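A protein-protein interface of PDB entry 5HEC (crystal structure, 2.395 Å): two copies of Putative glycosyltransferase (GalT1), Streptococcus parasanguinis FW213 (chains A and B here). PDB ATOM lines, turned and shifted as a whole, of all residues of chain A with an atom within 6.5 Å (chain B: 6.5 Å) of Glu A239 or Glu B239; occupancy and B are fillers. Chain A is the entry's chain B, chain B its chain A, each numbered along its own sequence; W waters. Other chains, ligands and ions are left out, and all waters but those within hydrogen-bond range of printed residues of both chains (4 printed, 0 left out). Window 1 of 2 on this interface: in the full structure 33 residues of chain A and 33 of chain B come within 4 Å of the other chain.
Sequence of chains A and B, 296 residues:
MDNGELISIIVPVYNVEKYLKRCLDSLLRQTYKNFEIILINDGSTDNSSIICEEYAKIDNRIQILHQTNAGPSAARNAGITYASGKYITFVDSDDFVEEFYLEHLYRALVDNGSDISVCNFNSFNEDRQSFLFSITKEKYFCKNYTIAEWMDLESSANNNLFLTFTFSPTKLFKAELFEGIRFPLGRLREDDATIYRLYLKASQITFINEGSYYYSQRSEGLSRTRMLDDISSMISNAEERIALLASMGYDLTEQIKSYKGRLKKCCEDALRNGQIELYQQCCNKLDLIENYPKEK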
ATOM      1  N   MET A 234     -20.330   5.189   3.126  1.00  0.00           N
ATOM      2  CA  MET A 234     -21.481   5.764   3.790  1.00  0.00           C
ATOM      3  C   MET A 234     -22.416   6.404   2.756  1.00  0.00           C
ATOM      4  O   MET A 234     -23.640   6.189   2.780  1.00  0.00           O
ATOM      5  CB  MET A 234     -21.021   6.789   4.839  1.00  0.00           C
ATOM      6  CG  MET A 234     -22.127   7.387   5.676  1.00  0.00           C
ATOM      7  SD  MET A 234     -21.490   8.526   6.930  1.00  0.00           S
ATOM      8  CE  MET A 234     -20.903   9.914   5.920  1.00  0.00           C
ATOM      9  N   ILE A 235     -21.826   7.165   1.839  1.00  0.00           N
ATOM     10  CA  ILE A 235     -22.595   7.877   0.832  1.00  0.00           C
ATOM     11  C   ILE A 235     -23.089   6.945  -0.281  1.00  0.00           C
ATOM     12  O   ILE A 235     -24.253   7.014  -0.675  1.00  0.00           O
ATOM     13  CB  ILE A 235     -21.772   9.012   0.208  1.00  0.00           C
ATOM     14  CG1 ILE A 235     -21.312   9.984   1.293  1.00  0.00           C
ATOM     15  CG2 ILE A 235     -22.588   9.746  -0.853  1.00  0.00           C
ATOM     16  CD1 ILE A 235     -22.471  10.545   2.089  1.00  0.00           C
ATOM     17  N   SER A 236     -22.225   6.072  -0.791  1.00  0.00           N
ATOM     18  CA  SER A 236     -22.635   5.261  -1.934  1.00  0.00           C
ATOM     19  C   SER A 236     -23.584   4.141  -1.501  1.00  0.00           C
ATOM     20  O   SER A 236     -24.430   3.723  -2.297  1.00  0.00           O
ATOM     21  CB  SER A 236     -21.426   4.689  -2.688  1.00  0.00           C
ATOM     22  OG  SER A 236     -20.678   3.818  -1.878  1.00  0.00           O
ATOM     23  N   ASN A 237     -23.468   3.680  -0.250  1.00  0.00           N
ATOM     24  CA  ASN A 237     -24.442   2.727   0.287  1.00  0.00           C
ATOM     25  C   ASN A 237     -25.835   3.343   0.320  1.00  0.00           C
ATOM     26  O   ASN A 237     -26.811   2.689  -0.060  1.00  0.00           O
ATOM     27  CB  ASN A 237     -24.079   2.260   1.703  1.00  0.00           C
ATOM     28  CG  ASN A 237     -22.929   1.273   1.727  1.00  0.00           C
ATOM     29  OD1 ASN A 237     -22.474   0.804   0.686  1.00  0.00           O
ATOM     30  ND2 ASN A 237     -22.459   0.947   2.925  1.00  0.00           N
ATOM     31  N   ALA A 238     -25.920   4.597   0.782  1.00  0.00           N
ATOM     32  CA  ALA A 238     -27.212   5.289   0.859  1.00  0.00           C
ATOM     33  C   ALA A 238     -27.815   5.529  -0.544  1.00  0.00           C
ATOM     34  O   ALA A 238     -29.021   5.367  -0.739  1.00  0.00           O
ATOM     35  CB  ALA A 238     -27.071   6.601   1.607  1.00  0.00           C
ATOM     36  N   GLU A 239     -26.976   5.893  -1.517  1.00  0.00           N
ATOM     37  CA  GLU A 239     -27.449   6.117  -2.890  1.00  0.00           C
ATOM     38  C   GLU A 239     -27.976   4.832  -3.530  1.00  0.00           C
ATOM     39  O   GLU A 239     -29.037   4.811  -4.146  1.00  0.00           O
ATOM     40  CB  GLU A 239     -26.330   6.737  -3.738  1.00  0.00           C
ATOM     41  CG  GLU A 239     -26.065   8.201  -3.338  1.00  0.00           C
ATOM     42  CD  GLU A 239     -24.691   8.746  -3.771  1.00  0.00           C
ATOM     43  OE1 GLU A 239     -23.836   7.963  -4.282  1.00  0.00           O
ATOM     44  OE2 GLU A 239     -24.480   9.976  -3.586  1.00  0.00           O
ATOM     45  N   GLU A 240     -27.229   3.756  -3.349  1.00  0.00           N
ATOM     46  CA  GLU A 240     -27.609   2.446  -3.827  1.00  0.00           C
ATOM     47  C   GLU A 240     -28.948   1.997  -3.219  1.00  0.00           C
ATOM     48  O   GLU A 240     -29.844   1.524  -3.920  1.00  0.00           O
ATOM     49  CB  GLU A 240     -26.492   1.453  -3.486  1.00  0.00           C
ATOM     50  CG  GLU A 240     -26.750   0.015  -3.835  1.00  0.00           C
ATOM     51  CD  GLU A 240     -25.486  -0.837  -3.633  1.00  0.00           C
ATOM     52  OE1 GLU A 240     -25.010  -0.948  -2.474  1.00  0.00           O
ATOM     53  OE2 GLU A 240     -24.944  -1.356  -4.638  1.00  0.00           O
ATOM     54  N   ARG A 241     -29.079   2.160  -1.909  1.00  0.00           N
ATOM     55  CA  ARG A 241     -30.292   1.737  -1.237  1.00  0.00           C
ATOM     56  C   ARG A 241     -31.486   2.544  -1.756  1.00  0.00           C
ATOM     57  O   ARG A 241     -32.553   1.979  -2.019  1.00  0.00           O
ATOM     58  CB  ARG A 241     -30.147   1.873   0.281  1.00  0.00           C
ATOM     59  CG  ARG A 241     -31.433   1.626   1.052  1.00  0.00           C
ATOM     60  CD  ARG A 241     -31.155   1.337   2.511  1.00  0.00           C
ATOM     61  NE  ARG A 241     -30.280   2.332   3.115  1.00  0.00           N
ATOM     62  CZ  ARG A 241     -29.033   2.094   3.526  1.00  0.00           C
ATOM     63  NH1 ARG A 241     -28.499   0.877   3.416  1.00  0.00           N
ATOM     64  NH2 ARG A 241     -28.320   3.080   4.064  1.00  0.00           N
ATOM     65  N   ILE A 242     -31.300   3.849  -1.939  1.00  0.00           N
ATOM     66  CA  ILE A 242     -32.402   4.676  -2.395  1.00  0.00           C
ATOM     67  C   ILE A 242     -32.796   4.250  -3.807  1.00  0.00           C
ATOM     68  O   ILE A 242     -33.980   4.154  -4.113  1.00  0.00           O
ATOM     69  CB  ILE A 242     -32.055   6.181  -2.353  1.00  0.00           C
ATOM     70  CG1 ILE A 242     -32.054   6.688  -0.910  1.00  0.00           C
ATOM     71  CG2 ILE A 242     -33.043   6.996  -3.175  1.00  0.00           C
ATOM     72  CD1 ILE A 242     -31.558   8.141  -0.758  1.00  0.00           C
ATOM     73  N   ALA A 243     -31.810   3.958  -4.653  1.00  0.00           N
ATOM     74  CA  ALA A 243     -32.106   3.584  -6.036  1.00  0.00           C
ATOM     75  C   ALA A 243     -32.886   2.269  -6.102  1.00  0.00           C
ATOM     76  O   ALA A 243     -33.834   2.136  -6.872  1.00  0.00           O
ATOM     77  CB  ALA A 243     -30.825   3.482  -6.846  1.00  0.00           C
ATOM     78  N   LEU A 244     -32.493   1.302  -5.281  1.00  0.00           N
ATOM     79  CA  LEU A 244     -33.186   0.027  -5.218  1.00  0.00           C
ATOM     80  C   LEU A 244     -34.636   0.158  -4.756  1.00  0.00           C
ATOM     81  O   LEU A 244     -35.545  -0.357  -5.392  1.00  0.00           O
ATOM     82  CB  LEU A 244     -32.450  -0.917  -4.275  1.00  0.00           C
ATOM     83  CG  LEU A 244     -31.616  -2.013  -4.911  1.00  0.00           C
ATOM     84  CD1 LEU A 244     -31.059  -2.878  -3.774  1.00  0.00           C
ATOM     85  CD2 LEU A 244     -32.442  -2.850  -5.925  1.00  0.00           C
ATOM     86  N   TYR A 259     -30.009  10.174   4.032  1.00  0.00           N
ATOM     87  CA  TYR A 259     -29.036  10.562   3.003  1.00  0.00           C
ATOM     88  C   TYR A 259     -28.507  11.986   3.195  1.00  0.00           C
ATOM     89  O   TYR A 259     -27.294  12.202   3.151  1.00  0.00           O
ATOM     90  CB  TYR A 259     -29.671  10.412   1.607  1.00  0.00           C
ATOM     91  CG  TYR A 259     -28.788  10.771   0.416  1.00  0.00           C
ATOM     92  CD1 TYR A 259     -27.490  10.274   0.294  1.00  0.00           C
ATOM     93  CD2 TYR A 259     -29.287  11.555  -0.621  1.00  0.00           C
ATOM     94  CE1 TYR A 259     -26.709  10.583  -0.805  1.00  0.00           C
ATOM     95  CE2 TYR A 259     -28.519  11.862  -1.725  1.00  0.00           C
ATOM     96  CZ  TYR A 259     -27.235  11.380  -1.813  1.00  0.00           C
ATOM     97  OH  TYR A 259     -26.489  11.703  -2.921  1.00  0.00           O
ATOM     98  N   LEU A 263     -24.642  13.245   4.041  1.00  0.00           N
ATOM     99  CA  LEU A 263     -23.964  14.223   3.203  1.00  0.00           C
ATOM    100  C   LEU A 263     -23.322  15.328   4.039  1.00  0.00           C
ATOM    101  O   LEU A 263     -22.153  15.667   3.821  1.00  0.00           O
ATOM    102  CB  LEU A 263     -24.940  14.812   2.181  1.00  0.00           C
ATOM    103  CG  LEU A 263     -25.220  13.839   1.034  1.00  0.00           C
ATOM    104  CD1 LEU A 263     -26.422  14.281   0.177  1.00  0.00           C
ATOM    105  CD2 LEU A 263     -23.952  13.697   0.190  1.00  0.00           C
ATOM    106  N   LYS A 285     -23.405  17.860  -3.865  1.00  0.00           N
ATOM    107  CA  LYS A 285     -24.679  17.192  -3.665  1.00  0.00           C
ATOM    108  C   LYS A 285     -25.518  17.905  -2.595  1.00  0.00           C
ATOM    109  O   LYS A 285     -26.715  18.132  -2.783  1.00  0.00           O
ATOM    110  CB  LYS A 285     -24.457  15.711  -3.309  1.00  0.00           C
ATOM    111  CG  LYS A 285     -23.982  14.887  -4.504  1.00  0.00           C
ATOM    112  CD  LYS A 285     -23.961  13.388  -4.252  1.00  0.00           C
ATOM    113  CE  LYS A 285     -22.532  12.877  -4.250  1.00  0.00           C
ATOM    114  NZ  LYS A 285     -22.444  11.392  -4.195  1.00  0.00           N
ATOM    115  N   SER B 232     -18.850  -0.638 -13.652  1.00  0.00           N
ATOM    116  CA  SER B 232     -19.041  -0.187 -12.284  1.00  0.00           C
ATOM    117  C   SER B 232     -19.633   1.236 -12.203  1.00  0.00           C
ATOM    118  O   SER B 232     -20.657   1.452 -11.546  1.00  0.00           O
ATOM    119  CB  SER B 232     -17.713  -0.247 -11.540  1.00  0.00           C
ATOM    120  OG  SER B 232     -17.908   0.051 -10.183  1.00  0.00           O
ATOM    121  N   MET B 234     -21.126   2.906 -14.498  1.00  0.00           N
ATOM    122  CA  MET B 234     -22.428   2.911 -15.138  1.00  0.00           C
ATOM    123  C   MET B 234     -23.525   2.719 -14.079  1.00  0.00           C
ATOM    124  O   MET B 234     -24.558   3.400 -14.087  1.00  0.00           O
ATOM    125  CB  MET B 234     -22.483   1.817 -16.216  1.00  0.00           C
ATOM    126  CG  MET B 234     -23.762   1.769 -17.039  1.00  0.00           C
ATOM    127  SD  MET B 234     -23.756   0.408 -18.237  1.00  0.00           S
ATOM    128  CE  MET B 234     -23.790  -1.048 -17.162  1.00  0.00           C
ATOM    129  N   ILE B 235     -23.280   1.804 -13.157  1.00  0.00           N
ATOM    130  CA  ILE B 235     -24.259   1.495 -12.135  1.00  0.00           C
ATOM    131  C   ILE B 235     -24.278   2.564 -11.038  1.00  0.00           C
ATOM    132  O   ILE B 235     -25.349   3.034 -10.639  1.00  0.00           O
ATOM    133  CB  ILE B 235     -23.982   0.126 -11.514  1.00  0.00           C
ATOM    134  CG1 ILE B 235     -23.994  -0.944 -12.607  1.00  0.00           C
ATOM    135  CG2 ILE B 235     -24.999  -0.179 -10.435  1.00  0.00           C
ATOM    136  CD1 ILE B 235     -25.280  -0.928 -13.421  1.00  0.00           C
ATOM    137  N   SER B 236     -23.100   2.961 -10.559  1.00  0.00           N
ATOM    138  CA  SER B 236     -23.049   3.874  -9.422  1.00  0.00           C
ATOM    139  C   SER B 236     -23.466   5.297  -9.829  1.00  0.00           C
ATOM    140  O   SER B 236     -24.094   6.001  -9.031  1.00  0.00           O
ATOM    141  CB  SER B 236     -21.656   3.873  -8.776  1.00  0.00           C
ATOM    142  OG  SER B 236     -20.684   4.313  -9.696  1.00  0.00           O
ATOM    143  N   ASN B 237     -23.144   5.711 -11.056  1.00  0.00           N
ATOM    144  CA  ASN B 237     -23.648   6.986 -11.564  1.00  0.00           C
ATOM    145  C   ASN B 237     -25.178   7.021 -11.557  1.00  0.00           C
ATOM    146  O   ASN B 237     -25.771   8.030 -11.167  1.00  0.00           O
ATOM    147  CB  ASN B 237     -23.163   7.270 -12.989  1.00  0.00           C
ATOM    148  CG  ASN B 237     -21.675   7.594 -13.065  1.00  0.00           C
ATOM    149  OD1 ASN B 237     -21.015   7.819 -12.058  1.00  0.00           O
ATOM    150  ND2 ASN B 237     -21.149   7.623 -14.281  1.00  0.00           N
ATOM    151  N   ALA B 238     -25.811   5.928 -11.998  1.00  0.00           N
ATOM    152  CA  ALA B 238     -27.276   5.866 -12.044  1.00  0.00           C
ATOM    153  C   ALA B 238     -27.879   5.905 -10.622  1.00  0.00           C
ATOM    154  O   ALA B 238     -28.888   6.562 -10.391  1.00  0.00           O
ATOM    155  CB  ALA B 238     -27.741   4.619 -12.787  1.00  0.00           C
ATOM    156  N   GLU B 239     -27.243   5.218  -9.671  1.00  0.00           N
ATOM    157  CA  GLU B 239     -27.727   5.209  -8.287  1.00  0.00           C
ATOM    158  C   GLU B 239     -27.626   6.586  -7.626  1.00  0.00           C
ATOM    159  O   GLU B 239     -28.544   7.042  -6.937  1.00  0.00           O
ATOM    160  CB  GLU B 239     -26.962   4.151  -7.479  1.00  0.00           C
ATOM    161  CG  GLU B 239     -27.411   2.730  -7.861  1.00  0.00           C
ATOM    162  CD  GLU B 239     -26.426   1.623  -7.473  1.00  0.00           C
ATOM    163  OE1 GLU B 239     -25.281   1.932  -7.037  1.00  0.00           O
ATOM    164  OE2 GLU B 239     -26.814   0.430  -7.624  1.00  0.00           O
ATOM    165  N   GLU B 240     -26.506   7.249  -7.863  1.00  0.00           N
ATOM    166  CA  GLU B 240     -26.259   8.573  -7.346  1.00  0.00           C
ATOM    167  C   GLU B 240     -27.245   9.594  -7.944  1.00  0.00           C
ATOM    168  O   GLU B 240     -27.771  10.455  -7.239  1.00  0.00           O
ATOM    169  CB  GLU B 240     -24.806   8.947  -7.648  1.00  0.00           C
ATOM    170  CG  GLU B 240     -24.418  10.386  -7.442  1.00  0.00           C
ATOM    171  CD  GLU B 240     -22.900  10.570  -7.579  1.00  0.00           C
ATOM    172  OE1 GLU B 240     -22.358  10.486  -8.714  1.00  0.00           O
ATOM    173  OE2 GLU B 240     -22.241  10.760  -6.533  1.00  0.00           O
ATOM    174  N   ARG B 241     -27.507   9.483  -9.240  1.00  0.00           N
ATOM    175  CA  ARG B 241     -28.422  10.409  -9.889  1.00  0.00           C
ATOM    176  C   ARG B 241     -29.838  10.208  -9.332  1.00  0.00           C
ATOM    177  O   ARG B 241     -30.535  11.182  -9.040  1.00  0.00           O
ATOM    178  CB  ARG B 241     -28.386  10.235 -11.414  1.00  0.00           C
ATOM    179  CG  ARG B 241     -29.479  10.981 -12.167  1.00  0.00           C
ATOM    180  CD  ARG B 241     -29.164  11.091 -13.654  1.00  0.00           C
ATOM    181  NE  ARG B 241     -28.786   9.811 -14.241  1.00  0.00           N
ATOM    182  CZ  ARG B 241     -27.569   9.525 -14.715  1.00  0.00           C
ATOM    183  NH1 ARG B 241     -26.599  10.436 -14.688  1.00  0.00           N
ATOM    184  NH2 ARG B 241     -27.318   8.323 -15.227  1.00  0.00           N
ATOM    185  N   ILE B 242     -30.243   8.953  -9.141  1.00  0.00           N
ATOM    186  CA  ILE B 242     -31.576   8.695  -8.634  1.00  0.00           C
ATOM    187  C   ILE B 242     -31.706   9.240  -7.210  1.00  0.00           C
ATOM    188  O   ILE B 242     -32.697   9.899  -6.892  1.00  0.00           O
ATOM    189  CB  ILE B 242     -31.921   7.193  -8.685  1.00  0.00           C
ATOM    190  CG1 ILE B 242     -32.119   6.751 -10.140  1.00  0.00           C
ATOM    191  CG2 ILE B 242     -33.183   6.897  -7.886  1.00  0.00           C
ATOM    192  CD1 ILE B 242     -32.371   5.246 -10.323  1.00  0.00           C
ATOM    193  N   ALA B 243     -30.697   9.017  -6.372  1.00  0.00           N
ATOM    194  CA  ALA B 243     -30.749   9.499  -4.991  1.00  0.00           C
ATOM    195  C   ALA B 243     -30.864  11.020  -4.919  1.00  0.00           C
ATOM    196  O   ALA B 243     -31.615  11.562  -4.109  1.00  0.00           O
ATOM    197  CB  ALA B 243     -29.533   9.037  -4.222  1.00  0.00           C
ATOM    198  N   LEU B 244     -30.113  11.709  -5.772  1.00  0.00           N
ATOM    199  CA  LEU B 244     -30.147  13.161  -5.824  1.00  0.00           C
ATOM    200  C   LEU B 244     -31.509  13.701  -6.274  1.00  0.00           C
ATOM    201  O   LEU B 244     -32.088  14.572  -5.638  1.00  0.00           O
ATOM    202  CB  LEU B 244     -29.075  13.666  -6.780  1.00  0.00           C
ATOM    203  CG  LEU B 244     -27.820  14.294  -6.212  1.00  0.00           C
ATOM    204  CD1 LEU B 244     -27.041  14.875  -7.393  1.00  0.00           C
ATOM    205  CD2 LEU B 244     -28.154  15.383  -5.168  1.00  0.00           C
ATOM    206  N   TYR B 259     -32.061   2.690 -15.139  1.00  0.00           N
ATOM    207  CA  TYR B 259     -31.323   1.931 -14.129  1.00  0.00           C
ATOM    208  C   TYR B 259     -31.489   0.414 -14.299  1.00  0.00           C
ATOM    209  O   TYR B 259     -30.500  -0.328 -14.274  1.00  0.00           O
ATOM    210  CB  TYR B 259     -31.781   2.378 -12.729  1.00  0.00           C
ATOM    211  CG  TYR B 259     -31.122   1.675 -11.558  1.00  0.00           C
ATOM    212  CD1 TYR B 259     -29.739   1.570 -11.460  1.00  0.00           C
ATOM    213  CD2 TYR B 259     -31.892   1.156 -10.521  1.00  0.00           C
ATOM    214  CE1 TYR B 259     -29.142   0.941 -10.371  1.00  0.00           C
ATOM    215  CE2 TYR B 259     -31.306   0.534  -9.429  1.00  0.00           C
ATOM    216  CZ  TYR B 259     -29.943   0.431  -9.361  1.00  0.00           C
ATOM    217  OH  TYR B 259     -29.387  -0.186  -8.274  1.00  0.00           O
ATOM    218  N   LEU B 263     -28.628  -2.370 -15.207  1.00  0.00           N
ATOM    219  CA  LEU B 263     -28.417  -3.564 -14.403  1.00  0.00           C
ATOM    220  C   LEU B 263     -28.380  -4.834 -15.251  1.00  0.00           C
ATOM    221  O   LEU B 263     -27.529  -5.694 -15.028  1.00  0.00           O
ATOM    222  CB  LEU B 263     -29.494  -3.668 -13.326  1.00  0.00           C
ATOM    223  CG  LEU B 263     -29.225  -2.664 -12.203  1.00  0.00           C
ATOM    224  CD1 LEU B 263     -30.435  -2.502 -11.277  1.00  0.00           C
ATOM    225  CD2 LEU B 263     -27.990  -3.101 -11.426  1.00  0.00           C
ATOM    226  N   LYS B 285     -29.270  -7.151  -7.348  1.00  0.00           N
ATOM    227  CA  LYS B 285     -30.129  -5.984  -7.509  1.00  0.00           C
ATOM    228  C   LYS B 285     -31.232  -6.240  -8.548  1.00  0.00           C
ATOM    229  O   LYS B 285     -32.401  -5.885  -8.333  1.00  0.00           O
ATOM    230  CB  LYS B 285     -29.294  -4.751  -7.886  1.00  0.00           C
ATOM    231  CG  LYS B 285     -28.500  -4.183  -6.714  1.00  0.00           C
ATOM    232  CD  LYS B 285     -27.822  -2.859  -7.043  1.00  0.00           C
ATOM    233  CE  LYS B 285     -26.307  -2.994  -7.001  1.00  0.00           C
ATOM    234  NZ  LYS B 285     -25.578  -1.685  -7.036  1.00  0.00           N
HETATM  235  O   HOH W   1     -23.343   0.155  -7.246  1.00  0.00           O
HETATM  236  O   HOH W   2     -21.379   8.718  -4.223  1.00  0.00           O
HETATM  237  O   HOH W   3     -23.715   3.536  -5.385  1.00  0.00           O
HETATM  238  O   HOH W   4     -23.230   5.928  -5.934  1.00  0.00           O
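Glu A239 touches Ala B243, and with the chains exchanged Ala A243 touches Glu B239. Glu A240 touches Lys B285, and with the chains exchanged Lys A285 touches Glu B240. Ile A242 touches Ala B243, and with the chains exchanged Ala A243 touches Ile B242. Ala A243 touches Tyr B259, and with the chains exchanged Tyr A259 touches Ala B243.
NZ of Lys B285 lies within salt-bridge range of OE2 of Glu B239. The side-chain carboxylate (OE2) of Glu A239 lies within hydrogen-bond range of the side-chain hydroxyl (OH) of Tyr A259 (2.7 Å). OE2 of Glu B239 sits at hydrogen-bond distance from OH of Tyr B259, at 2.7 Å. The side-chain amino group of Lys A285 lies within salt-bridge range of the side-chain carboxylate of Glu A239, at 2.6 Å.
The side-chain carboxylate (OE2) of Glu A240 is in salt-bridge range of the side-chain amino group (NZ) of Lys B285 (2.5 Å). OE2 of Glu B240 is in salt-bridge range of NZ of Lys A285.
Of chain B, only Glu B239, Glu B240 and Ala B243 come within 4 Å of Glu A239. Of the printed residues of chain B, Glu A240 touches Glu B239 (3.8 Å) and Lys B285 (2.5 Å). Arg A241 touches none of the printed residues of chain B. Printed residues of chain B within 4 Å of Ile A242: Ala B243. Glu B239 touches just these residues of chain A: Glu A239, Glu A240 and Ala A243. Of the printed residues of chain A, Ile B242 touches Ala A243 (3.9 Å). Leu B263 touches none of the printed residues of chain A. The nearest residue of chain A that does not touch Glu B239 is Ser A236 (5.1 Å).
Among the printed residues, pairs that only touch across the chains: Glu A239 with Glu B239 (3.6 Å), Glu A239 with Glu B240 (3.6 Å), Ala A243 with Glu B239 (3.6 Å), Glu A239 with Ala B243 (3.7 Å), Glu A240 with Glu B239 (3.8 Å), Ile A242 with Ala B243 (3.9 Å), Leu A244 with Lys B285 (3.9 Å), Tyr A259 with Ala B243 (3.9 Å), Lys A285 with Leu B244 (3.9 Å), Ala A243 with Tyr B259 (3.9 Å) and Ala A243 with Ile B242 (3.9 Å).
Hydrophobic or aromatic side chains of chain A within 4 Å of the printed part of chain B: Ile A242, Ala A243, Leu A244 and Tyr A259. Among the printed residues, Asp or Glu carboxylates within 4 Å of a Lys or Arg side-chain nitrogen of the other chain: Glu A240 with Lys B285 (2.5 Å) and Lys A285 with Glu B240 (2.4 Å).
Water W2 lies within hydrogen-bond range of OE1 of Glu A239, NZ of Lys A285 and OE2 of Glu B240. Water W1 lies within hydrogen-bond range of the side-chain carboxylate of Glu B239 (2.6 Å), the side-chain amino group of Lys B285 (2.9 Å) and the side-chain carboxylate of Glu A240 (3.4 Å). Water W4 bridges the side-chain carboxylate of Glu A239 (2.7 Å) and the backbone carbonyl oxygen of Ser B236 (3.2 Å). Water W3 lies within hydrogen-bond range of the side-chain carboxylate (OE1) of Glu B239 (2.8 Å) and the backbone carbonyl oxygen (O) of Ser A236 (3.2 Å).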
